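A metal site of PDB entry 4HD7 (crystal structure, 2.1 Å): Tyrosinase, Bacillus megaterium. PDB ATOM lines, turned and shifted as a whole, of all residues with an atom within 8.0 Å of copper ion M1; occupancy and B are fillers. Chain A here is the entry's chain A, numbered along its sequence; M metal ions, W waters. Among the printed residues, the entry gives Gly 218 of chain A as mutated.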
ATOM      1  N   HIS A  42      30.756   2.307  -8.583  1.00  0.00           N
ATOM      2  CA  HIS A  42      29.635   3.247  -8.637  1.00  0.00           C
ATOM      3  C   HIS A  42      28.437   2.698  -9.410  1.00  0.00           C
ATOM      4  O   HIS A  42      27.294   2.800  -8.946  1.00  0.00           O
ATOM      5  CB  HIS A  42      30.091   4.578  -9.244  1.00  0.00           C
ATOM      6  CG  HIS A  42      29.091   5.672  -9.080  1.00  0.00           C
ATOM      7  ND1 HIS A  42      28.110   5.911 -10.013  1.00  0.00           N
ATOM      8  CD2 HIS A  42      28.920   6.602  -8.112  1.00  0.00           C
ATOM      9  CE1 HIS A  42      27.381   6.946  -9.634  1.00  0.00           C
ATOM     10  NE2 HIS A  42      27.857   7.391  -8.474  1.00  0.00           N
ATOM     11  N   GLY A  43      28.678   2.130 -10.592  1.00  0.00           N
ATOM     12  CA  GLY A  43      27.600   1.532 -11.373  1.00  0.00           C
ATOM     13  C   GLY A  43      26.925   0.388 -10.639  1.00  0.00           C
ATOM     14  O   GLY A  43      25.700   0.342 -10.515  1.00  0.00           O
ATOM     15  N   ALA A  45      26.791  -0.107  -7.540  1.00  0.00           N
ATOM     16  CA  ALA A  45      26.119   0.303  -6.311  1.00  0.00           C
ATOM     17  C   ALA A  45      24.728   0.816  -6.623  1.00  0.00           C
ATOM     18  O   ALA A  45      23.777   0.501  -5.911  1.00  0.00           O
ATOM     19  CB  ALA A  45      26.933   1.368  -5.552  1.00  0.00           C
ATOM     20  N   GLY A  46      24.600   1.569  -7.717  1.00  0.00           N
ATOM     21  CA  GLY A  46      23.358   2.236  -8.053  1.00  0.00           C
ATOM     22  C   GLY A  46      22.300   1.270  -8.516  1.00  0.00           C
ATOM     23  O   GLY A  46      21.114   1.598  -8.504  1.00  0.00           O
ATOM     24  N   ASN A  57      18.979   2.848  -3.416  1.00  0.00           N
ATOM     25  CA  ASN A  57      20.081   1.940  -3.701  1.00  0.00           C
ATOM     26  C   ASN A  57      21.199   2.239  -2.730  1.00  0.00           C
ATOM     27  O   ASN A  57      21.108   3.180  -1.947  1.00  0.00           O
ATOM     28  CB  ASN A  57      20.544   2.007  -5.176  1.00  0.00           C
ATOM     29  CG  ASN A  57      21.023   3.392  -5.613  1.00  0.00           C
ATOM     30  OD1 ASN A  57      20.302   4.117  -6.315  1.00  0.00           O
ATOM     31  ND2 ASN A  57      22.242   3.740  -5.256  1.00  0.00           N
ATOM     32  N   ALA A  59      24.065   3.544  -2.964  1.00  0.00           N
ATOM     33  CA  ALA A  59      24.867   4.750  -3.132  1.00  0.00           C
ATOM     34  C   ALA A  59      24.069   6.044  -3.294  1.00  0.00           C
ATOM     35  O   ALA A  59      24.665   7.118  -3.284  1.00  0.00           O
ATOM     36  CB  ALA A  59      25.835   4.574  -4.300  1.00  0.00           C
ATOM     37  N   HIS A  60      22.758   5.938  -3.438  1.00  0.00           N
ATOM     38  CA  HIS A  60      21.917   7.122  -3.730  1.00  0.00           C
ATOM     39  C   HIS A  60      20.483   7.008  -3.227  1.00  0.00           C
ATOM     40  O   HIS A  60      19.983   5.914  -2.951  1.00  0.00           O
ATOM     41  CB  HIS A  60      21.879   7.396  -5.233  1.00  0.00           C
ATOM     42  CG  HIS A  60      23.232   7.415  -5.885  1.00  0.00           C
ATOM     43  ND1 HIS A  60      23.776   6.306  -6.486  1.00  0.00           N
ATOM     44  CD2 HIS A  60      24.145   8.412  -6.025  1.00  0.00           C
ATOM     45  CE1 HIS A  60      24.977   6.613  -6.972  1.00  0.00           C
ATOM     46  NE2 HIS A  60      25.203   7.882  -6.717  1.00  0.00           N
ATOM     47  N   PHE A  65      23.725   7.597   1.077  1.00  0.00           N
ATOM     48  CA  PHE A  65      24.292   8.494   0.081  1.00  0.00           C
ATOM     49  C   PHE A  65      25.577   9.172   0.543  1.00  0.00           C
ATOM     50  O   PHE A  65      26.617   9.038  -0.117  1.00  0.00           O
ATOM     51  CB  PHE A  65      23.250   9.556  -0.345  1.00  0.00           C
ATOM     52  CG  PHE A  65      23.797  10.624  -1.235  1.00  0.00           C
ATOM     53  CD1 PHE A  65      24.414  10.312  -2.438  1.00  0.00           C
ATOM     54  CD2 PHE A  65      23.706  11.947  -0.872  1.00  0.00           C
ATOM     55  CE1 PHE A  65      24.915  11.311  -3.258  1.00  0.00           C
ATOM     56  CE2 PHE A  65      24.207  12.946  -1.681  1.00  0.00           C
ATOM     57  CZ  PHE A  65      24.798  12.623  -2.884  1.00  0.00           C
ATOM     58  N   TRP A  68      28.429   6.533   1.830  1.00  0.00           N
ATOM     59  CA  TRP A  68      28.887   5.810   0.633  1.00  0.00           C
ATOM     60  C   TRP A  68      29.989   6.572  -0.105  1.00  0.00           C
ATOM     61  O   TRP A  68      31.107   6.078  -0.278  1.00  0.00           O
ATOM     62  CB  TRP A  68      27.724   5.508  -0.336  1.00  0.00           C
ATOM     63  CG  TRP A  68      28.075   4.417  -1.338  1.00  0.00           C
ATOM     64  CD1 TRP A  68      27.810   3.076  -1.222  1.00  0.00           C
ATOM     65  CD2 TRP A  68      28.783   4.566  -2.583  1.00  0.00           C
ATOM     66  NE1 TRP A  68      28.290   2.387  -2.319  1.00  0.00           N
ATOM     67  CE2 TRP A  68      28.896   3.278  -3.167  1.00  0.00           C
ATOM     68  CE3 TRP A  68      29.319   5.658  -3.272  1.00  0.00           C
ATOM     69  CZ2 TRP A  68      29.528   3.057  -4.389  1.00  0.00           C
ATOM     70  CZ3 TRP A  68      29.942   5.441  -4.503  1.00  0.00           C
ATOM     71  CH2 TRP A  68      30.044   4.147  -5.046  1.00  0.00           C
ATOM     72  N   HIS A  69      29.681   7.806  -0.514  1.00  0.00           N
ATOM     73  CA  HIS A  69      30.627   8.567  -1.304  1.00  0.00           C
ATOM     74  C   HIS A  69      31.852   8.964  -0.496  1.00  0.00           C
ATOM     75  O   HIS A  69      32.954   8.987  -1.034  1.00  0.00           O
ATOM     76  CB  HIS A  69      29.961   9.788  -1.985  1.00  0.00           C
ATOM     77  CG  HIS A  69      28.987   9.409  -3.057  1.00  0.00           C
ATOM     78  ND1 HIS A  69      27.662   9.100  -2.785  1.00  0.00           N
ATOM     79  CD2 HIS A  69      29.135   9.215  -4.382  1.00  0.00           C
ATOM     80  CE1 HIS A  69      27.051   8.765  -3.904  1.00  0.00           C
ATOM     81  NE2 HIS A  69      27.919   8.845  -4.900  1.00  0.00           N
ATOM     82  N   TYR A  72      33.983   6.082  -0.751  1.00  0.00           N
ATOM     83  CA  TYR A  72      34.397   5.995  -2.168  1.00  0.00           C
ATOM     84  C   TYR A  72      35.592   6.931  -2.415  1.00  0.00           C
ATOM     85  O   TYR A  72      36.592   6.532  -3.010  1.00  0.00           O
ATOM     86  CB  TYR A  72      33.205   6.343  -3.057  1.00  0.00           C
ATOM     87  CG  TYR A  72      33.379   6.270  -4.581  1.00  0.00           C
ATOM     88  CD1 TYR A  72      33.267   5.055  -5.261  1.00  0.00           C
ATOM     89  CD2 TYR A  72      33.548   7.428  -5.348  1.00  0.00           C
ATOM     90  CE1 TYR A  72      33.367   4.991  -6.660  1.00  0.00           C
ATOM     91  CE2 TYR A  72      33.666   7.378  -6.728  1.00  0.00           C
ATOM     92  CZ  TYR A  72      33.564   6.159  -7.389  1.00  0.00           C
ATOM     93  OH  TYR A  72      33.683   6.086  -8.769  1.00  0.00           O
ATOM     94  N   GLU A 195      21.287  16.142  -1.215  1.00  0.00           N
ATOM     95  CA  GLU A 195      21.287  15.274  -2.382  1.00  0.00           C
ATOM     96  C   GLU A 195      20.499  15.953  -3.483  1.00  0.00           C
ATOM     97  O   GLU A 195      20.786  15.810  -4.664  1.00  0.00           O
ATOM     98  CB  GLU A 195      20.694  13.893  -2.049  1.00  0.00           C
ATOM     99  CG  GLU A 195      20.756  12.912  -3.213  1.00  0.00           C
ATOM    100  CD  GLU A 195      20.501  11.446  -2.800  1.00  0.00           C
ATOM    101  OE1 GLU A 195      20.825  10.549  -3.634  1.00  0.00           O
ATOM    102  OE2 GLU A 195      19.993  11.193  -1.669  1.00  0.00           O
ATOM    103  N   HIS A 204      23.314  18.836  -5.032  1.00  0.00           N
ATOM    104  CA  HIS A 204      24.079  17.765  -5.624  1.00  0.00           C
ATOM    105  C   HIS A 204      23.526  17.322  -6.990  1.00  0.00           C
ATOM    106  O   HIS A 204      24.225  17.385  -7.977  1.00  0.00           O
ATOM    107  CB  HIS A 204      24.183  16.558  -4.682  1.00  0.00           C
ATOM    108  CG  HIS A 204      24.599  15.308  -5.351  1.00  0.00           C
ATOM    109  ND1 HIS A 204      23.685  14.380  -5.840  1.00  0.00           N
ATOM    110  CD2 HIS A 204      25.824  14.804  -5.650  1.00  0.00           C
ATOM    111  CE1 HIS A 204      24.341  13.377  -6.384  1.00  0.00           C
ATOM    112  NE2 HIS A 204      25.636  13.608  -6.276  1.00  0.00           N
ATOM    113  N   HIS A 208      25.044  17.729 -11.256  1.00  0.00           N
ATOM    114  CA  HIS A 208      25.168  16.667 -12.285  1.00  0.00           C
ATOM    115  C   HIS A 208      24.393  17.061 -13.535  1.00  0.00           C
ATOM    116  O   HIS A 208      24.888  16.939 -14.656  1.00  0.00           O
ATOM    117  CB  HIS A 208      24.627  15.308 -11.794  1.00  0.00           C
ATOM    118  CG  HIS A 208      25.548  14.606 -10.841  1.00  0.00           C
ATOM    119  ND1 HIS A 208      26.646  13.895 -11.260  1.00  0.00           N
ATOM    120  CD2 HIS A 208      25.495  14.478  -9.489  1.00  0.00           C
ATOM    121  CE1 HIS A 208      27.258  13.375 -10.205  1.00  0.00           C
ATOM    122  NE2 HIS A 208      26.592  13.719  -9.128  1.00  0.00           N
ATOM    123  N   GLY A 218      23.755   8.993 -13.752  1.00  0.00           N
ATOM    124  CA  GLY A 218      24.460   8.424 -12.623  1.00  0.00           C
ATOM    125  C   GLY A 218      25.501   7.378 -12.968  1.00  0.00           C
ATOM    126  O   GLY A 218      26.676   7.550 -12.655  1.00  0.00           O
ATOM    127  N   PRO A 219      25.069   6.306 -13.637  1.00  0.00           N
ATOM    128  CA  PRO A 219      25.901   5.153 -14.025  1.00  0.00           C
ATOM    129  C   PRO A 219      27.219   5.489 -14.736  1.00  0.00           C
ATOM    130  O   PRO A 219      28.127   4.670 -14.727  1.00  0.00           O
ATOM    131  CB  PRO A 219      24.997   4.376 -14.991  1.00  0.00           C
ATOM    132  CG  PRO A 219      23.640   4.696 -14.550  1.00  0.00           C
ATOM    133  CD  PRO A 219      23.694   6.153 -14.140  1.00  0.00           C
ATOM    134  N   ALA A 221      28.653   8.801 -14.557  1.00  0.00           N
ATOM    135  CA  ALA A 221      29.199  10.000 -13.941  1.00  0.00           C
ATOM    136  C   ALA A 221      30.723  10.006 -13.720  1.00  0.00           C
ATOM    137  O   ALA A 221      31.401  10.930 -14.171  1.00  0.00           O
ATOM    138  CB  ALA A 221      28.435  10.307 -12.639  1.00  0.00           C
ATOM    139  N   PRO A 222      31.267   8.965 -13.068  1.00  0.00           N
ATOM    140  CA  PRO A 222      32.687   8.960 -12.702  1.00  0.00           C
ATOM    141  C   PRO A 222      33.669   8.843 -13.869  1.00  0.00           C
ATOM    142  O   PRO A 222      34.882   8.989 -13.639  1.00  0.00           O
ATOM    143  CB  PRO A 222      32.823   7.750 -11.742  1.00  0.00           C
ATOM    144  CG  PRO A 222      31.396   7.407 -11.336  1.00  0.00           C
ATOM    145  CD  PRO A 222      30.548   7.798 -12.532  1.00  0.00           C
ATOM    146  N   PHE A 227      33.921  14.393 -11.410  1.00  0.00           N
ATOM    147  CA  PHE A 227      33.027  13.685 -10.491  1.00  0.00           C
ATOM    148  C   PHE A 227      33.530  13.684  -9.065  1.00  0.00           C
ATOM    149  O   PHE A 227      32.743  13.808  -8.118  1.00  0.00           O
ATOM    150  CB  PHE A 227      32.821  12.237 -10.952  1.00  0.00           C
ATOM    151  CG  PHE A 227      31.999  11.412 -10.011  1.00  0.00           C
ATOM    152  CD1 PHE A 227      32.582  10.742  -8.949  1.00  0.00           C
ATOM    153  CD2 PHE A 227      30.626  11.267 -10.203  1.00  0.00           C
ATOM    154  CE1 PHE A 227      31.816   9.960  -8.089  1.00  0.00           C
ATOM    155  CE2 PHE A 227      29.855  10.477  -9.363  1.00  0.00           C
ATOM    156  CZ  PHE A 227      30.446   9.825  -8.301  1.00  0.00           C
ATOM    157  N   HIS A 231      32.174  15.543  -5.715  1.00  0.00           N
ATOM    158  CA  HIS A 231      31.889  14.819  -4.488  1.00  0.00           C
ATOM    159  C   HIS A 231      32.754  15.232  -3.310  1.00  0.00           C
ATOM    160  O   HIS A 231      32.315  15.147  -2.177  1.00  0.00           O
ATOM    161  CB  HIS A 231      31.813  13.304  -4.698  1.00  0.00           C
ATOM    162  CG  HIS A 231      30.452  12.864  -5.159  1.00  0.00           C
ATOM    163  ND1 HIS A 231      29.446  12.549  -4.283  1.00  0.00           N
ATOM    164  CD2 HIS A 231      29.931  12.795  -6.406  1.00  0.00           C
ATOM    165  CE1 HIS A 231      28.351  12.238  -4.986  1.00  0.00           C
ATOM    166  NE2 HIS A 231      28.626  12.393  -6.258  1.00  0.00           N
HETATM  167 CU    CU M   1      27.115   8.422  -6.753  1.00  0.00          CU
HETATM  168 CU    CU M   2      26.689  12.303  -7.310  1.00  0.00          CU
HETATM  169  O   HOH W   1      26.755  10.125  -7.777  1.00  0.00           O
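A ring nitrogen (ND1) of His 69 is in hydrogen-bond range of the backbone carbonyl oxygen (O) of Phe 65 (2.9 Å). The side-chain amide nitrogen (ND2) of Asn 57 sits close to the backbone NH (N) of His 60, at 2.9 Å. The backbone carbonyl oxygen (O) of Gly 218 sits close to a ring nitrogen (ND1) of His 42.
Phe 227 touches copper ion M1. Four residues have an atom within 4 Å of copper ion M1: His 42, His 60, His 69 and Phe 227. The nearest printed residue that does not touch copper ion M1 is His 231 (4.3 Å).
Copper ion M1 is bound by a ring nitrogen (NE2) of His 60 (2.0 Å), water W1 (2.0 Å), a ring nitrogen (NE2) of His 69 (2.1 Å) and a ring nitrogen (NE2) of His 42 (2.1 Å). Copper ion M1 has four donor atoms within binding distance.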
